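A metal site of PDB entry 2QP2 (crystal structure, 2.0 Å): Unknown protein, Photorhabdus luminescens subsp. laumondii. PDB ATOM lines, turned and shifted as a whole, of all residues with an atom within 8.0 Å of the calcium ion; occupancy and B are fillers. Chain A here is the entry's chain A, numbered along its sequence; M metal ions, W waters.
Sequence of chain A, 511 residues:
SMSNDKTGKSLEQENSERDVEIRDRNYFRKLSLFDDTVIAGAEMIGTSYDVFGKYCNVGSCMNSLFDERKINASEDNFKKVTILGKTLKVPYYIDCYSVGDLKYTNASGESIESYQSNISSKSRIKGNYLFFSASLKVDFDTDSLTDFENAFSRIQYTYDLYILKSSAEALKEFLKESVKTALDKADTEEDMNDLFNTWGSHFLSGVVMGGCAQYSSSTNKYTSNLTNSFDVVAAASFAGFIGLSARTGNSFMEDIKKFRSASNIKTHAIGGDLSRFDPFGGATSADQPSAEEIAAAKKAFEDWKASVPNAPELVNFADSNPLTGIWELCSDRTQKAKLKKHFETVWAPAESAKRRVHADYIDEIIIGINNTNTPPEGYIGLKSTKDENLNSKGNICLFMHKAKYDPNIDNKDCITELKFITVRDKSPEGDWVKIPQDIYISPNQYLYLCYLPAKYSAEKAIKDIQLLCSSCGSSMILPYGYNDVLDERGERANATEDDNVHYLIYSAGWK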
ATOM      1  N   GLN A 437       5.104 -17.707   9.207  1.00  0.00           N
ATOM      2  CA  GLN A 437       5.901 -17.324   8.031  1.00  0.00           C
ATOM      3  C   GLN A 437       6.913 -16.217   8.303  1.00  0.00           C
ATOM      4  O   GLN A 437       6.561 -15.121   8.712  1.00  0.00           O
ATOM      5  CB  GLN A 437       5.006 -16.948   6.843  1.00  0.00           C
ATOM      6  CG  GLN A 437       5.770 -16.471   5.603  1.00  0.00           C
ATOM      7  CD  GLN A 437       6.523 -17.574   4.881  1.00  0.00           C
ATOM      8  OE1 GLN A 437       5.954 -18.606   4.538  1.00  0.00           O
ATOM      9  NE2 GLN A 437       7.812 -17.356   4.649  1.00  0.00           N
ATOM     10  N   ASP A 438       8.185 -16.531   8.056  1.00  0.00           N
ATOM     11  CA  ASP A 438       9.263 -15.546   8.063  1.00  0.00           C
ATOM     12  C   ASP A 438       9.052 -14.599   6.873  1.00  0.00           C
ATOM     13  O   ASP A 438       9.112 -15.032   5.717  1.00  0.00           O
ATOM     14  CB  ASP A 438      10.628 -16.253   7.991  1.00  0.00           C
ATOM     15  CG  ASP A 438      11.814 -15.295   8.053  1.00  0.00           C
ATOM     16  OD1 ASP A 438      11.635 -14.066   8.209  1.00  0.00           O
ATOM     17  OD2 ASP A 438      12.953 -15.792   7.933  1.00  0.00           O
ATOM     18  N   ILE A 439       8.790 -13.334   7.162  1.00  0.00           N
ATOM     19  CA  ILE A 439       8.497 -12.321   6.141  1.00  0.00           C
ATOM     20  C   ILE A 439       9.740 -11.981   5.309  1.00  0.00           C
ATOM     21  O   ILE A 439       9.634 -11.658   4.113  1.00  0.00           O
ATOM     22  CB  ILE A 439       7.870 -11.053   6.790  1.00  0.00           C
ATOM     23  CG1 ILE A 439       6.512 -11.394   7.396  1.00  0.00           C
ATOM     24  CG2 ILE A 439       7.744  -9.894   5.770  1.00  0.00           C
ATOM     25  CD1 ILE A 439       6.063 -10.449   8.510  1.00  0.00           C
ATOM     26  N   TYR A 440      10.914 -12.066   5.932  1.00  0.00           N
ATOM     27  CA  TYR A 440      12.190 -11.816   5.257  1.00  0.00           C
ATOM     28  C   TYR A 440      12.740 -13.094   4.648  1.00  0.00           C
ATOM     29  O   TYR A 440      13.088 -14.034   5.375  1.00  0.00           O
ATOM     30  CB  TYR A 440      13.223 -11.256   6.247  1.00  0.00           C
ATOM     31  CG  TYR A 440      13.032  -9.821   6.681  1.00  0.00           C
ATOM     32  CD1 TYR A 440      13.698  -9.333   7.807  1.00  0.00           C
ATOM     33  CD2 TYR A 440      12.198  -8.946   5.976  1.00  0.00           C
ATOM     34  CE1 TYR A 440      13.547  -8.013   8.229  1.00  0.00           C
ATOM     35  CE2 TYR A 440      12.042  -7.622   6.385  1.00  0.00           C
ATOM     36  CZ  TYR A 440      12.711  -7.164   7.508  1.00  0.00           C
ATOM     37  OH  TYR A 440      12.575  -5.857   7.934  1.00  0.00           O
ATOM     38  N   ILE A 441      12.823 -13.142   3.319  1.00  0.00           N
ATOM     39  CA  ILE A 441      13.359 -14.344   2.662  1.00  0.00           C
ATOM     40  C   ILE A 441      14.891 -14.434   2.697  1.00  0.00           C
ATOM     41  O   ILE A 441      15.474 -15.477   2.389  1.00  0.00           O
ATOM     42  CB  ILE A 441      12.814 -14.565   1.216  1.00  0.00           C
ATOM     43  CG1 ILE A 441      13.308 -13.480   0.266  1.00  0.00           C
ATOM     44  CG2 ILE A 441      11.275 -14.665   1.237  1.00  0.00           C
ATOM     45  CD1 ILE A 441      13.459 -13.952  -1.177  1.00  0.00           C
ATOM     46  N   SER A 442      15.555 -13.337   3.085  1.00  0.00           N
ATOM     47  CA  SER A 442      16.989 -13.372   3.350  1.00  0.00           C
ATOM     48  C   SER A 442      17.287 -14.428   4.411  1.00  0.00           C
ATOM     49  O   SER A 442      16.583 -14.500   5.419  1.00  0.00           O
ATOM     50  CB  SER A 442      17.494 -11.999   3.824  1.00  0.00           C
ATOM     51  OG  SER A 442      18.841 -12.084   4.259  1.00  0.00           O
ATOM     52  N   PRO A 443      18.328 -15.255   4.183  1.00  0.00           N
ATOM     53  CA  PRO A 443      18.657 -16.343   5.111  1.00  0.00           C
ATOM     54  C   PRO A 443      19.241 -15.895   6.458  1.00  0.00           C
ATOM     55  O   PRO A 443      19.230 -16.670   7.411  1.00  0.00           O
ATOM     56  CB  PRO A 443      19.696 -17.166   4.334  1.00  0.00           C
ATOM     57  CG  PRO A 443      20.322 -16.211   3.390  1.00  0.00           C
ATOM     58  CD  PRO A 443      19.233 -15.232   3.023  1.00  0.00           C
ATOM     59  N   ASN A 444      19.739 -14.665   6.544  1.00  0.00           N
ATOM     60  CA  ASN A 444      20.335 -14.164   7.790  1.00  0.00           C
ATOM     61  C   ASN A 444      19.497 -13.107   8.526  1.00  0.00           C
ATOM     62  O   ASN A 444      19.979 -12.441   9.442  1.00  0.00           O
ATOM     63  CB  ASN A 444      21.779 -13.670   7.562  1.00  0.00           C
ATOM     64  CG  ASN A 444      21.926 -12.827   6.299  1.00  0.00           C
ATOM     65  OD1 ASN A 444      21.146 -11.901   6.048  1.00  0.00           O
ATOM     66  ND2 ASN A 444      22.946 -13.142   5.504  1.00  0.00           N
ATOM     67  N   GLN A 445      18.230 -12.972   8.105  1.00  0.00           N
ATOM     68  CA  GLN A 445      17.301 -12.001   8.687  1.00  0.00           C
ATOM     69  C   GLN A 445      15.938 -12.646   8.937  1.00  0.00           C
ATOM     70  O   GLN A 445      15.473 -13.469   8.137  1.00  0.00           O
ATOM     71  CB  GLN A 445      17.125 -10.809   7.735  1.00  0.00           C
ATOM     72  CG  GLN A 445      18.377  -9.960   7.529  1.00  0.00           C
ATOM     73  CD  GLN A 445      18.633  -8.979   8.665  1.00  0.00           C
ATOM     74  OE1 GLN A 445      19.741  -8.916   9.216  1.00  0.00           O
ATOM     75  NE2 GLN A 445      17.611  -8.202   9.030  1.00  0.00           N
ATOM     76  N   TYR A 446      15.302 -12.282  10.048  1.00  0.00           N
ATOM     77  CA  TYR A 446      13.990 -12.820  10.421  1.00  0.00           C
ATOM     78  C   TYR A 446      12.996 -11.709  10.748  1.00  0.00           C
ATOM     79  O   TYR A 446      13.364 -10.715  11.384  1.00  0.00           O
ATOM     80  CB  TYR A 446      14.105 -13.762  11.625  1.00  0.00           C
ATOM     81  CG  TYR A 446      14.999 -14.967  11.392  1.00  0.00           C
ATOM     82  CD1 TYR A 446      14.459 -16.199  11.020  1.00  0.00           C
ATOM     83  CD2 TYR A 446      16.386 -14.884  11.574  1.00  0.00           C
ATOM     84  CE1 TYR A 446      15.275 -17.308  10.817  1.00  0.00           C
ATOM     85  CE2 TYR A 446      17.201 -15.980  11.369  1.00  0.00           C
ATOM     86  CZ  TYR A 446      16.639 -17.192  10.989  1.00  0.00           C
ATOM     87  OH  TYR A 446      17.460 -18.278  10.793  1.00  0.00           O
ATOM     88  N   LEU A 447      11.750 -11.899  10.321  1.00  0.00           N
ATOM     89  CA  LEU A 447      10.646 -11.010  10.692  1.00  0.00           C
ATOM     90  C   LEU A 447       9.334 -11.786  10.739  1.00  0.00           C
ATOM     91  O   LEU A 447       8.886 -12.327   9.722  1.00  0.00           O
ATOM     92  CB  LEU A 447      10.525  -9.826   9.719  1.00  0.00           C
ATOM     93  CG  LEU A 447       9.504  -8.731  10.086  1.00  0.00           C
ATOM     94  CD1 LEU A 447      10.013  -7.840  11.210  1.00  0.00           C
ATOM     95  CD2 LEU A 447       9.141  -7.891   8.869  1.00  0.00           C
ATOM     96  N   TYR A 448       8.737 -11.852  11.929  1.00  0.00           N
ATOM     97  CA  TYR A 448       7.463 -12.524  12.128  1.00  0.00           C
ATOM     98  C   TYR A 448       6.450 -11.547  12.694  1.00  0.00           C
ATOM     99  O   TYR A 448       6.750 -10.813  13.637  1.00  0.00           O
ATOM    100  CB  TYR A 448       7.605 -13.699  13.102  1.00  0.00           C
ATOM    101  CG  TYR A 448       8.649 -14.735  12.738  1.00  0.00           C
ATOM    102  CD1 TYR A 448       8.335 -15.786  11.875  1.00  0.00           C
ATOM    103  CD2 TYR A 448       9.933 -14.681  13.270  1.00  0.00           C
ATOM    104  CE1 TYR A 448       9.296 -16.748  11.544  1.00  0.00           C
ATOM    105  CE2 TYR A 448      10.884 -15.634  12.947  1.00  0.00           C
ATOM    106  CZ  TYR A 448      10.561 -16.663  12.088  1.00  0.00           C
ATOM    107  OH  TYR A 448      11.505 -17.610  11.762  1.00  0.00           O
ATOM    108  N   GLU A 497      12.012  -6.245   1.094  1.00  0.00           N
ATOM    109  CA  GLU A 497      13.459  -6.453   1.002  1.00  0.00           C
ATOM    110  C   GLU A 497      14.112  -5.893  -0.264  1.00  0.00           C
ATOM    111  O   GLU A 497      15.326  -6.006  -0.435  1.00  0.00           O
ATOM    112  CB  GLU A 497      13.793  -7.936   1.150  1.00  0.00           C
ATOM    113  CG  GLU A 497      13.728  -8.445   2.580  1.00  0.00           C
ATOM    114  CD  GLU A 497      13.936  -9.941   2.666  1.00  0.00           C
ATOM    115  OE1 GLU A 497      13.211 -10.691   1.973  1.00  0.00           O
ATOM    116  OE2 GLU A 497      14.830 -10.373   3.431  1.00  0.00           O
HETATM  117 CA    CA M   1      14.716 -15.088   6.656  1.00  0.00          CA
HETATM  118  O   HOH W   1      16.350 -16.239   7.956  1.00  0.00           O
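The side-chain amide oxygen of Asn 444 sits at hydrogen-bond distance from the side-chain hydroxyl of Ser 442. The backbone NH (N) of Ser 442 lies within hydrogen-bond range of the side-chain carboxylate (OE2) of Glu 497 (3.1 Å). The side-chain carboxylate (OD1) of Asp 438 sits at hydrogen-bond distance from the backbone NH (N) of Leu 447 (3.0 Å).
Of the 13 residues printed, 4 come within 4 Å of the calcium ion. The nearest printed residue that does not touch the calcium ion is Ile 441 (4.02 Å).
The calcium ion is bound by the side-chain carboxylate of Asp 438 (2.3 Å), the backbone carbonyl oxygen of Ser 442 (2.3 Å), the backbone carbonyl oxygen of Gln 445 (2.3 Å), the backbone carbonyl oxygen of Tyr 440 (2.3 Å) and water W1 (2.4 Å). The calcium ion has five donor atoms within binding distance.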
